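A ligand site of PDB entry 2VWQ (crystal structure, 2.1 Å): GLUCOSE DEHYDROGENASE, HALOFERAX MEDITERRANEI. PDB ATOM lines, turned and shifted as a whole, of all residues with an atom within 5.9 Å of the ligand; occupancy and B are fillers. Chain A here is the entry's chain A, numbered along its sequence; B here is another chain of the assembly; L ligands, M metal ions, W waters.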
ATOM      1  N   ASP A  38       4.033 -21.809 -13.356  1.00  0.00           N
ATOM      2  CA  ASP A  38       4.998 -22.701 -14.024  1.00  0.00           C
ATOM      3  C   ASP A  38       6.458 -22.471 -13.567  1.00  0.00           C
ATOM      4  O   ASP A  38       6.700 -21.722 -12.603  1.00  0.00           O
ATOM      5  CB  ASP A  38       4.802 -22.814 -15.571  1.00  0.00           C
ATOM      6  CG  ASP A  38       5.460 -21.716 -16.380  1.00  0.00           C
ATOM      7  OD1 ASP A  38       6.202 -20.885 -15.863  1.00  0.00           O
ATOM      8  OD2 ASP A  38       5.206 -21.655 -17.591  1.00  0.00           O
ATOM      9  N   GLY A  39       7.380 -23.183 -14.223  1.00  0.00           N
ATOM     10  CA  GLY A  39       8.808 -23.135 -13.908  1.00  0.00           C
ATOM     11  C   GLY A  39       9.354 -21.732 -13.797  1.00  0.00           C
ATOM     12  O   GLY A  39      10.123 -21.422 -12.893  1.00  0.00           O
ATOM     13  N   THR A  40       8.891 -20.867 -14.704  1.00  0.00           N
ATOM     14  CA  THR A  40       9.351 -19.493 -14.734  1.00  0.00           C
ATOM     15  C   THR A  40       9.029 -18.736 -13.461  1.00  0.00           C
ATOM     16  O   THR A  40       9.821 -17.916 -13.020  1.00  0.00           O
ATOM     17  CB  THR A  40       8.752 -18.784 -15.980  1.00  0.00           C
ATOM     18  OG1 THR A  40       9.009 -19.573 -17.155  1.00  0.00           O
ATOM     19  CG2 THR A  40       9.343 -17.417 -16.164  1.00  0.00           C
ATOM     20  N   ILE A 154       1.829 -21.384 -26.395  1.00  0.00           N
ATOM     21  CA  ILE A 154       3.263 -21.532 -26.568  1.00  0.00           C
ATOM     22  C   ILE A 154       3.531 -22.619 -27.617  1.00  0.00           C
ATOM     23  O   ILE A 154       4.276 -22.421 -28.580  1.00  0.00           O
ATOM     24  CB  ILE A 154       3.972 -21.865 -25.227  1.00  0.00           C
ATOM     25  CG1 ILE A 154       3.910 -20.665 -24.227  1.00  0.00           C
ATOM     26  CG2 ILE A 154       5.428 -22.255 -25.446  1.00  0.00           C
ATOM     27  CD1 ILE A 154       4.538 -19.347 -24.737  1.00  0.00           C
ATOM     28  N   LEU A 179      10.524 -34.195 -25.618  1.00  0.00           N
ATOM     29  CA  LEU A 179      11.560 -34.286 -24.622  1.00  0.00           C
ATOM     30  C   LEU A 179      11.106 -33.517 -23.407  1.00  0.00           C
ATOM     31  O   LEU A 179      10.945 -32.292 -23.459  1.00  0.00           O
ATOM     32  CB  LEU A 179      12.893 -33.744 -25.145  1.00  0.00           C
ATOM     33  CG  LEU A 179      13.316 -34.191 -26.536  1.00  0.00           C
ATOM     34  CD1 LEU A 179      14.658 -33.560 -26.906  1.00  0.00           C
ATOM     35  CD2 LEU A 179      13.401 -35.688 -26.655  1.00  0.00           C
ATOM     36  N   GLY A 180      10.866 -34.242 -22.316  1.00  0.00           N
ATOM     37  CA  GLY A 180      10.461 -33.615 -21.054  1.00  0.00           C
ATOM     38  C   GLY A 180       9.043 -33.941 -20.658  1.00  0.00           C
ATOM     39  O   GLY A 180       8.146 -33.917 -21.485  1.00  0.00           O
ATOM     40  N   ASN A 181       8.852 -34.181 -19.356  1.00  0.00           N
ATOM     41  CA  ASN A 181       7.587 -34.640 -18.787  1.00  0.00           C
ATOM     42  C   ASN A 181       7.067 -33.645 -17.758  1.00  0.00           C
ATOM     43  O   ASN A 181       6.422 -34.020 -16.765  1.00  0.00           O
ATOM     44  CB  ASN A 181       7.745 -36.039 -18.160  1.00  0.00           C
ATOM     45  CG  ASN A 181       8.825 -36.086 -17.064  1.00  0.00           C
ATOM     46  OD1 ASN A 181       9.915 -35.497 -17.201  1.00  0.00           O
ATOM     47  ND2 ASN A 181       8.529 -36.792 -15.975  1.00  0.00           N
ATOM     48  N   GLY A 182       7.376 -32.379 -17.997  1.00  0.00           N
ATOM     49  CA  GLY A 182       6.819 -31.268 -17.243  1.00  0.00           C
ATOM     50  C   GLY A 182       5.481 -30.908 -17.835  1.00  0.00           C
ATOM     51  O   GLY A 182       5.012 -31.559 -18.756  1.00  0.00           O
ATOM     52  N   SER A 183       4.863 -29.876 -17.297  1.00  0.00           N
ATOM     53  CA  SER A 183       3.508 -29.512 -17.702  1.00  0.00           C
ATOM     54  C   SER A 183       3.459 -29.101 -19.198  1.00  0.00           C
ATOM     55  O   SER A 183       2.517 -29.464 -19.876  1.00  0.00           O
ATOM     56  CB  SER A 183       2.939 -28.408 -16.809  1.00  0.00           C
ATOM     57  OG  SER A 183       3.743 -27.252 -16.884  1.00  0.00           O
ATOM     58  N   LEU A 184       4.481 -28.413 -19.698  1.00  0.00           N
ATOM     59  CA  LEU A 184       4.564 -28.087 -21.132  1.00  0.00           C
ATOM     60  C   LEU A 184       4.734 -29.315 -22.030  1.00  0.00           C
ATOM     61  O   LEU A 184       4.104 -29.422 -23.062  1.00  0.00           O
ATOM     62  CB  LEU A 184       5.700 -27.088 -21.428  1.00  0.00           C
ATOM     63  CG  LEU A 184       5.717 -26.477 -22.843  1.00  0.00           C
ATOM     64  CD1 LEU A 184       4.414 -25.699 -23.142  1.00  0.00           C
ATOM     65  CD2 LEU A 184       6.954 -25.617 -23.092  1.00  0.00           C
ATOM     66  N   GLY A 185       5.666 -30.203 -21.679  1.00  0.00           N
ATOM     67  CA  GLY A 185       5.856 -31.436 -22.427  1.00  0.00           C
ATOM     68  C   GLY A 185       4.611 -32.306 -22.459  1.00  0.00           C
ATOM     69  O   GLY A 185       4.226 -32.805 -23.525  1.00  0.00           O
ATOM     70  N   LEU A 205      10.147 -38.348 -23.345  1.00  0.00           N
ATOM     71  CA  LEU A 205      11.362 -38.541 -22.577  1.00  0.00           C
ATOM     72  C   LEU A 205      11.227 -38.008 -21.165  1.00  0.00           C
ATOM     73  O   LEU A 205      10.800 -36.860 -20.959  1.00  0.00           O
ATOM     74  CB  LEU A 205      12.536 -37.792 -23.232  1.00  0.00           C
ATOM     75  CG  LEU A 205      13.926 -38.129 -22.686  1.00  0.00           C
ATOM     76  CD1 LEU A 205      14.502 -39.325 -23.397  1.00  0.00           C
ATOM     77  CD2 LEU A 205      14.867 -36.953 -22.807  1.00  0.00           C
ATOM     78  N   GLY A 206      11.656 -38.816 -20.203  1.00  0.00           N
ATOM     79  CA  GLY A 206      11.731 -38.395 -18.799  1.00  0.00           C
ATOM     80  C   GLY A 206      12.819 -39.178 -18.086  1.00  0.00           C
ATOM     81  O   GLY A 206      13.617 -39.876 -18.719  1.00  0.00           O
ATOM     82  N   ARG A 207      12.853 -39.066 -16.757  1.00  0.00           N
ATOM     83  CA  ARG A 207      13.861 -39.792 -15.959  1.00  0.00           C
ATOM     84  C   ARG A 207      13.306 -40.130 -14.573  1.00  0.00           C
ATOM     85  O   ARG A 207      13.967 -39.898 -13.568  1.00  0.00           O
ATOM     86  CB  ARG A 207      15.121 -38.932 -15.844  1.00  0.00           C
ATOM     87  CG  ARG A 207      14.899 -37.524 -15.262  1.00  0.00           C
ATOM     88  CD  ARG A 207      16.185 -36.752 -15.186  1.00  0.00           C
ATOM     89  NE  ARG A 207      15.987 -35.427 -14.621  1.00  0.00           N
ATOM     90  CZ  ARG A 207      16.901 -34.454 -14.646  1.00  0.00           C
ATOM     91  NH1 ARG A 207      18.097 -34.640 -15.196  1.00  0.00           N
ATOM     92  NH2 ARG A 207      16.615 -33.285 -14.111  1.00  0.00           N
ATOM     93  N   ARG A 208      12.082 -40.655 -14.541  1.00  0.00           N
ATOM     94  CA  ARG A 208      11.382 -41.013 -13.299  1.00  0.00           C
ATOM     95  C   ARG A 208      11.353 -42.513 -13.130  1.00  0.00           C
ATOM     96  O   ARG A 208      11.302 -43.256 -14.114  1.00  0.00           O
ATOM     97  CB  ARG A 208       9.943 -40.521 -13.330  1.00  0.00           C
ATOM     98  CG  ARG A 208       9.773 -39.022 -13.447  1.00  0.00           C
ATOM     99  CD  ARG A 208      10.207 -38.312 -12.198  1.00  0.00           C
ATOM    100  NE  ARG A 208      10.115 -36.865 -12.325  1.00  0.00           N
ATOM    101  CZ  ARG A 208       9.013 -36.147 -12.148  1.00  0.00           C
ATOM    102  NH1 ARG A 208       7.866 -36.705 -11.826  1.00  0.00           N
ATOM    103  NH2 ARG A 208       9.078 -34.835 -12.286  1.00  0.00           N
ATOM    104  N   SER A 228      15.545 -41.428 -19.971  1.00  0.00           N
ATOM    105  CA  SER A 228      16.831 -40.945 -20.522  1.00  0.00           C
ATOM    106  C   SER A 228      18.051 -41.560 -19.819  1.00  0.00           C
ATOM    107  O   SER A 228      19.140 -41.570 -20.391  1.00  0.00           O
ATOM    108  CB  SER A 228      16.925 -39.420 -20.468  1.00  0.00           C
ATOM    109  OG  SER A 228      16.927 -38.952 -19.137  1.00  0.00           O
ATOM    110  N   GLU A 248      11.472 -30.094 -27.903  1.00  0.00           N
ATOM    111  CA  GLU A 248      12.335 -30.047 -26.708  1.00  0.00           C
ATOM    112  C   GLU A 248      11.766 -29.106 -25.633  1.00  0.00           C
ATOM    113  O   GLU A 248      11.615 -27.909 -25.854  1.00  0.00           O
ATOM    114  CB  GLU A 248      13.765 -29.681 -27.104  1.00  0.00           C
ATOM    115  CG  GLU A 248      14.744 -29.486 -25.958  1.00  0.00           C
ATOM    116  CD  GLU A 248      14.624 -28.119 -25.306  1.00  0.00           C
ATOM    117  OE1 GLU A 248      14.534 -27.111 -26.037  1.00  0.00           O
ATOM    118  OE2 GLU A 248      14.567 -28.047 -24.060  1.00  0.00           O
ATOM    119  N   ALA A 249      11.459 -29.691 -24.476  1.00  0.00           N
ATOM    120  CA  ALA A 249      10.930 -28.980 -23.323  1.00  0.00           C
ATOM    121  C   ALA A 249      11.590 -29.445 -22.006  1.00  0.00           C
ATOM    122  O   ALA A 249      10.908 -29.624 -20.982  1.00  0.00           O
ATOM    123  CB  ALA A 249       9.405 -29.158 -23.250  1.00  0.00           C
ATOM    124  N   THR A 250      12.914 -29.638 -22.040  1.00  0.00           N
ATOM    125  CA  THR A 250      13.709 -30.030 -20.866  1.00  0.00           C
ATOM    126  C   THR A 250      14.600 -28.912 -20.347  1.00  0.00           C
ATOM    127  O   THR A 250      14.892 -28.859 -19.159  1.00  0.00           O
ATOM    128  CB  THR A 250      14.645 -31.204 -21.163  1.00  0.00           C
ATOM    129  OG1 THR A 250      15.536 -30.854 -22.216  1.00  0.00           O
ATOM    130  CG2 THR A 250      13.880 -32.454 -21.542  1.00  0.00           C
ATOM    131  N   GLY A 251      15.066 -28.034 -21.245  1.00  0.00           N
ATOM    132  CA  GLY A 251      15.996 -26.985 -20.866  1.00  0.00           C
ATOM    133  C   GLY A 251      17.392 -27.536 -20.674  1.00  0.00           C
ATOM    134  O   GLY A 251      18.241 -26.888 -20.098  1.00  0.00           O
ATOM    135  N   PHE A 252      17.625 -28.740 -21.201  1.00  0.00           N
ATOM    136  CA  PHE A 252      18.919 -29.400 -21.108  1.00  0.00           C
ATOM    137  C   PHE A 252      19.674 -29.276 -22.457  1.00  0.00           C
ATOM    138  O   PHE A 252      19.271 -29.883 -23.437  1.00  0.00           O
ATOM    139  CB  PHE A 252      18.675 -30.868 -20.744  1.00  0.00           C
ATOM    140  CG  PHE A 252      19.924 -31.628 -20.395  1.00  0.00           C
ATOM    141  CD1 PHE A 252      20.820 -31.138 -19.453  1.00  0.00           C
ATOM    142  CD2 PHE A 252      20.192 -32.852 -20.999  1.00  0.00           C
ATOM    143  CE1 PHE A 252      21.970 -31.858 -19.123  1.00  0.00           C
ATOM    144  CE2 PHE A 252      21.323 -33.576 -20.682  1.00  0.00           C
ATOM    145  CZ  PHE A 252      22.212 -33.084 -19.746  1.00  0.00           C
ATOM    146  N   HIS A 255      20.329 -31.964 -25.180  1.00  0.00           N
ATOM    147  CA  HIS A 255      19.184 -32.347 -26.008  1.00  0.00           C
ATOM    148  C   HIS A 255      19.062 -31.528 -27.279  1.00  0.00           C
ATOM    149  O   HIS A 255      18.711 -32.078 -28.326  1.00  0.00           O
ATOM    150  CB  HIS A 255      17.882 -32.293 -25.201  1.00  0.00           C
ATOM    151  CG  HIS A 255      17.805 -33.302 -24.107  1.00  0.00           C
ATOM    152  ND1 HIS A 255      16.933 -33.182 -23.041  1.00  0.00           N
ATOM    153  CD2 HIS A 255      18.485 -34.461 -23.906  1.00  0.00           C
ATOM    154  CE1 HIS A 255      17.080 -34.233 -22.248  1.00  0.00           C
ATOM    155  NE2 HIS A 255      18.016 -35.010 -22.752  1.00  0.00           N
ATOM    156  N   LEU A 271      12.745 -26.164 -30.440  1.00  0.00           N
ATOM    157  CA  LEU A 271      13.417 -25.962 -29.157  1.00  0.00           C
ATOM    158  C   LEU A 271      12.672 -24.901 -28.372  1.00  0.00           C
ATOM    159  O   LEU A 271      12.471 -23.784 -28.862  1.00  0.00           O
ATOM    160  CB  LEU A 271      14.855 -25.504 -29.363  1.00  0.00           C
ATOM    161  CG  LEU A 271      15.736 -26.417 -30.207  1.00  0.00           C
ATOM    162  CD1 LEU A 271      17.084 -25.725 -30.380  1.00  0.00           C
ATOM    163  CD2 LEU A 271      15.870 -27.807 -29.558  1.00  0.00           C
ATOM    164  N   LEU A 272      12.252 -25.271 -27.176  1.00  0.00           N
ATOM    165  CA  LEU A 272      11.519 -24.361 -26.275  1.00  0.00           C
ATOM    166  C   LEU A 272      12.228 -24.115 -24.935  1.00  0.00           C
ATOM    167  O   LEU A 272      11.854 -23.202 -24.206  1.00  0.00           O
ATOM    168  CB  LEU A 272      10.129 -24.930 -25.970  1.00  0.00           C
ATOM    169  CG  LEU A 272       8.997 -24.906 -27.019  1.00  0.00           C
ATOM    170  CD1 LEU A 272       8.549 -23.499 -27.336  1.00  0.00           C
ATOM    171  CD2 LEU A 272       9.381 -25.644 -28.281  1.00  0.00           C
ATOM    172  N   GLY A 273      13.228 -24.925 -24.612  1.00  0.00           N
ATOM    173  CA  GLY A 273      13.889 -24.848 -23.313  1.00  0.00           C
ATOM    174  C   GLY A 273      14.825 -23.662 -23.189  1.00  0.00           C
ATOM    175  O   GLY A 273      15.369 -23.172 -24.169  1.00  0.00           O
ATOM    176  N   VAL A 274      15.012 -23.189 -21.959  1.00  0.00           N
ATOM    177  CA  VAL A 274      15.827 -22.013 -21.700  1.00  0.00           C
ATOM    178  C   VAL A 274      16.888 -22.373 -20.677  1.00  0.00           C
ATOM    179  O   VAL A 274      16.650 -22.273 -19.485  1.00  0.00           O
ATOM    180  CB  VAL A 274      14.954 -20.848 -21.172  1.00  0.00           C
ATOM    181  CG1 VAL A 274      15.810 -19.595 -21.012  1.00  0.00           C
ATOM    182  CG2 VAL A 274      13.773 -20.580 -22.119  1.00  0.00           C
ATOM    183  N   PRO A 275      18.077 -22.813 -21.146  1.00  0.00           N
ATOM    184  CA  PRO A 275      19.130 -23.238 -20.247  1.00  0.00           C
ATOM    185  C   PRO A 275      20.095 -22.132 -19.911  1.00  0.00           C
ATOM    186  O   PRO A 275      20.127 -21.092 -20.587  1.00  0.00           O
ATOM    187  CB  PRO A 275      19.861 -24.263 -21.088  1.00  0.00           C
ATOM    188  CG  PRO A 275      19.785 -23.708 -22.465  1.00  0.00           C
ATOM    189  CD  PRO A 275      18.482 -22.944 -22.555  1.00  0.00           C
ATOM    190  N   SER A 301      11.577 -21.120 -30.480  1.00  0.00           N
ATOM    191  CA  SER A 301      10.339 -20.357 -30.322  1.00  0.00           C
ATOM    192  C   SER A 301      10.170 -19.916 -28.884  1.00  0.00           C
ATOM    193  O   SER A 301      10.445 -20.685 -27.955  1.00  0.00           O
ATOM    194  CB  SER A 301       9.138 -21.204 -30.730  1.00  0.00           C
ATOM    195  OG  SER A 301       7.957 -20.424 -30.790  1.00  0.00           O
ATOM    196  N   VAL A 302       9.727 -18.678 -28.705  1.00  0.00           N
ATOM    197  CA  VAL A 302       9.439 -18.179 -27.360  1.00  0.00           C
ATOM    198  C   VAL A 302       8.149 -17.379 -27.435  1.00  0.00           C
ATOM    199  O   VAL A 302       7.875 -16.755 -28.465  1.00  0.00           O
ATOM    200  CB  VAL A 302      10.605 -17.305 -26.764  1.00  0.00           C
ATOM    201  CG1 VAL A 302      10.827 -16.012 -27.548  1.00  0.00           C
ATOM    202  CG2 VAL A 302      10.323 -16.973 -25.319  1.00  0.00           C
ATOM    203  N   ASN A 303       7.365 -17.450 -26.363  1.00  0.00           N
ATOM    204  CA  ASN A 303       6.180 -16.601 -26.208  1.00  0.00           C
ATOM    205  C   ASN A 303       5.115 -16.977 -27.273  1.00  0.00           C
ATOM    206  O   ASN A 303       5.143 -18.079 -27.841  1.00  0.00           O
ATOM    207  CB  ASN A 303       6.628 -15.120 -26.247  1.00  0.00           C
ATOM    208  CG  ASN A 303       5.593 -14.164 -25.685  1.00  0.00           C
ATOM    209  OD1 ASN A 303       5.023 -13.360 -26.429  1.00  0.00           O
ATOM    210  ND2 ASN A 303       5.333 -14.251 -24.380  1.00  0.00           N
ATOM    211  N   ASP A 345       7.567 -34.704  -7.212  1.00  0.00           N
ATOM    212  CA  ASP A 345       7.344 -35.513  -8.391  1.00  0.00           C
ATOM    213  C   ASP A 345       5.862 -35.717  -8.713  1.00  0.00           C
ATOM    214  O   ASP A 345       5.496 -35.886  -9.881  1.00  0.00           O
ATOM    215  CB  ASP A 345       8.084 -36.851  -8.264  1.00  0.00           C
ATOM    216  CG  ASP A 345       9.604 -36.719  -8.457  1.00  0.00           C
ATOM    217  OD1 ASP A 345      10.101 -35.602  -8.760  1.00  0.00           O
ATOM    218  OD2 ASP A 345      10.308 -37.743  -8.323  1.00  0.00           O
ATOM    219  N   VAL B 292      16.329 -20.199 -28.862  1.00  0.00           N
ATOM    220  CA  VAL B 292      14.984 -20.088 -28.293  1.00  0.00           C
ATOM    221  C   VAL B 292      14.556 -18.652 -28.033  1.00  0.00           C
ATOM    222  O   VAL B 292      13.512 -18.213 -28.526  1.00  0.00           O
ATOM    223  CB  VAL B 292      14.849 -20.929 -27.025  1.00  0.00           C
ATOM    224  CG1 VAL B 292      13.499 -20.693 -26.358  1.00  0.00           C
ATOM    225  CG2 VAL B 292      15.044 -22.398 -27.396  1.00  0.00           C
HETATM  226  P1  LIG L   1       9.552 -28.209 -15.933  1.00  0.00           P
HETATM  227  O1  LIG L   1       8.319 -28.287 -15.139  1.00  0.00           O
HETATM  228  O2  LIG L   1      10.811 -27.975 -15.262  1.00  0.00           O
HETATM  229  O3  LIG L   1       9.688 -29.544 -16.794  1.00  0.00           O
HETATM  230  C1  LIG L   1      10.961 -29.944 -17.223  1.00  0.00           C
HETATM  231  C2  LIG L   1      10.976 -31.448 -17.208  1.00  0.00           C
HETATM  232  O4  LIG L   1      12.106 -31.877 -17.931  1.00  0.00           O
HETATM  233  C3  LIG L   1      11.066 -32.016 -15.784  1.00  0.00           C
HETATM  234  O5  LIG L   1       9.978 -32.874 -15.550  1.00  0.00           O
HETATM  235  C4  LIG L   1      12.396 -32.762 -15.797  1.00  0.00           C
HETATM  236  O6  LIG L   1      12.356 -33.981 -15.097  1.00  0.00           O
HETATM  237  C5  LIG L   1      12.624 -32.994 -17.283  1.00  0.00           C
HETATM  238  N1  LIG L   1      14.045 -33.147 -17.566  1.00  0.00           N
HETATM  239  C6  LIG L   1      15.061 -32.253 -17.340  1.00  0.00           C
HETATM  240  N2  LIG L   1      16.221 -32.833 -17.721  1.00  0.00           N
HETATM  241  C7  LIG L   1      15.934 -34.088 -18.174  1.00  0.00           C
HETATM  242  C8  LIG L   1      16.706 -35.087 -18.684  1.00  0.00           C
HETATM  243  N3  LIG L   1      18.019 -34.919 -18.800  1.00  0.00           N
HETATM  244  N4  LIG L   1      16.126 -36.268 -19.082  1.00  0.00           N
HETATM  245  C9  LIG L   1      14.766 -36.448 -18.976  1.00  0.00           C
HETATM  246  N5  LIG L   1      13.989 -35.440 -18.456  1.00  0.00           N
HETATM  247  C10 LIG L   1      14.563 -34.284 -18.077  1.00  0.00           C
HETATM  248  O7  LIG L   1       9.256 -27.039 -16.984  1.00  0.00           O
HETATM  249  P2  LIG L   1       8.016 -26.784 -17.976  1.00  0.00           P
HETATM  250  O8  LIG L   1       7.442 -28.047 -18.527  1.00  0.00           O
HETATM  251  O9  LIG L   1       7.055 -25.797 -17.418  1.00  0.00           O
HETATM  252  O10 LIG L   1       8.983 -26.074 -19.072  1.00  0.00           O
HETATM  253  C11 LIG L   1       9.972 -26.848 -19.723  1.00  0.00           C
HETATM  254  C12 LIG L   1      11.078 -25.981 -20.303  1.00  0.00           C
HETATM  255  O11 LIG L   1      10.492 -25.082 -21.234  1.00  0.00           O
HETATM  256  C13 LIG L   1      11.821 -25.100 -19.295  1.00  0.00           C
HETATM  257  O12 LIG L   1      13.179 -24.979 -19.657  1.00  0.00           O
HETATM  258  C14 LIG L   1      11.167 -23.751 -19.433  1.00  0.00           C
HETATM  259  O13 LIG L   1      12.052 -22.695 -19.148  1.00  0.00           O
HETATM  260  C15 LIG L   1      10.844 -23.747 -20.911  1.00  0.00           C
HETATM  261  N6  LIG L   1       9.733 -22.906 -21.350  1.00  0.00           N
HETATM  262  C16 LIG L   1       9.939 -22.130 -22.460  1.00  0.00           C
HETATM  263  C17 LIG L   1       8.900 -21.343 -22.938  1.00  0.00           C
HETATM  264  C18 LIG L   1       9.060 -20.638 -24.264  1.00  0.00           C
HETATM  265  O14 LIG L   1       8.146 -19.647 -24.580  1.00  0.00           O
HETATM  266  N7  LIG L   1      10.035 -20.977 -25.103  1.00  0.00           N
HETATM  267  C19 LIG L   1       7.666 -21.377 -22.302  1.00  0.00           C
HETATM  268  C20 LIG L   1       7.475 -22.205 -21.198  1.00  0.00           C
HETATM  269  C21 LIG L   1       8.528 -22.970 -20.733  1.00  0.00           C
HETATM  270  P3  LIG L   1      12.696 -34.075 -13.503  1.00  0.00           P
HETATM  271  O15 LIG L   1      11.608 -33.358 -12.806  1.00  0.00           O
HETATM  272  O16 LIG L   1      14.004 -33.395 -13.210  1.00  0.00           O
HETATM  273  O17 LIG L   1      12.708 -35.548 -13.201  1.00  0.00           O
HETATM  274 ZN    ZN M   1       3.410 -20.022 -19.118  1.00  0.00          ZN
HETATM  275  O   HOH W   1       8.288 -30.302 -19.934  1.00  0.00           O
HETATM  276  O   HOH W   2      19.743 -37.123 -20.579  1.00  0.00           O
HETATM  277  O   HOH W   3      11.604 -36.819 -15.458  1.00  0.00           O
HETATM  278  O   HOH W   4       5.371 -24.192 -18.991  1.00  0.00           O
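An oxygen (O16) of the ligand lies within salt-bridge range of the guanidinium group (NH2) of Arg 207.
A nitrogen (N4) of the ligand is in hydrogen-bond range of the side-chain hydroxyl (OG) of Ser 228.
The backbone carbonyl oxygen (O) of Leu 272 lies close to a nitrogen (N7) of the ligand.
O of Ser 301 sits at hydrogen-bond distance from N7 of the ligand.
N of Asn 303 is in hydrogen-bond range of O14 of the ligand (2.9 Å).
The guanidinium group (NH2) of Arg 208 is in salt-bridge range of an oxygen (O15) of the ligand, 3.0 Å away.
OD1 of Asn 181 is in hydrogen-bond range of O5 of the ligand (3.1 Å).
O8 of the ligand lies within hydrogen-bond range of N of Leu 184 (3.2 Å).
The backbone NH (N) of Ser 183 lies within hydrogen-bond range of an oxygen (O8) of the ligand (3.4 Å).
N of Val 274 lies within hydrogen-bond range of O12 of the ligand, 3.4 Å away.
The backbone carbonyl oxygen of Glu 248 is in hydrogen-bond range of the backbone NH of Leu 272, 3.0 Å away.
O of Leu 271 sits at hydrogen-bond distance from N of Ser 301, 3.2 Å away.
N of Ala 249 sits at hydrogen-bond distance from O of Leu 179 (2.8 Å).
A ring nitrogen (ND1) of His 255 is in hydrogen-bond range of the side-chain hydroxyl (OG1) of Thr 250 (2.8 Å).
The side-chain hydroxyl of Thr 250 sits at hydrogen-bond distance from the backbone NH of Phe 252.
OE1 of Glu 248 sits at hydrogen-bond distance from N of Gly 273 (2.9 Å).
The side-chain carboxylate (OE2) of Glu 248 is in hydrogen-bond range of the backbone NH (N) of Thr 250 (3.1 Å).
N of Gly 180 is in hydrogen-bond range of O of Leu 205 (2.9 Å).
CD1 of Ile 154 touches O14 of the ligand (3.6 Å).
CA of Gly 180 touches O4 of the ligand, 3.9 Å away.
Gly 182 touches the ligand.
Leu 205 touches the ligand (CD2 to C9, 3.9 Å).
C of Gly 206 touches C9 of the ligand, at 3.5 Å.
O of Ala 249 touches C11 of the ligand (3.2 Å).
CA of Thr 250 touches O4 of the ligand, at 3.8 Å.
CA of Gly 251 touches O12 of the ligand, 3.7 Å away.
Phe 252 touches the ligand (CD2 to N3, 3.7 Å).
His 255 touches the ligand (CE1 to N3, 3.6 Å).
Gly 273 touches the ligand (CA to O12, 3.7 Å).
Val 302 touches the ligand.
Val 292 of chain B touches the ligand (CG1 to N7, 3.7 Å).
Of the 32 residues printed, 23 come within 4 Å of the ligand.
Along chain A the residues within 4 Å of the ligand span positions 154 to 303.
Water W1 lies within hydrogen-bond range of an oxygen (O8) of the ligand, the backbone carbonyl oxygen (O) of Ala 249, the backbone NH (N) of Gly 182 and the backbone NH (N) of Gly 185.
Water W4 bridges O9 of the ligand (2.8 Å) and OD2 of Asp 38 (2.9 Å).
Water W3 lies within hydrogen-bond range of OD1 of Asn 181 (2.8 Å), O17 of the ligand (2.8 Å), N of Arg 207 (2.9 Å) and NE of Arg 208 (3.5 Å).
Water W2 bridges N3 of the ligand (3.3 Å) and NE2 of His 255 (3.5 Å).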
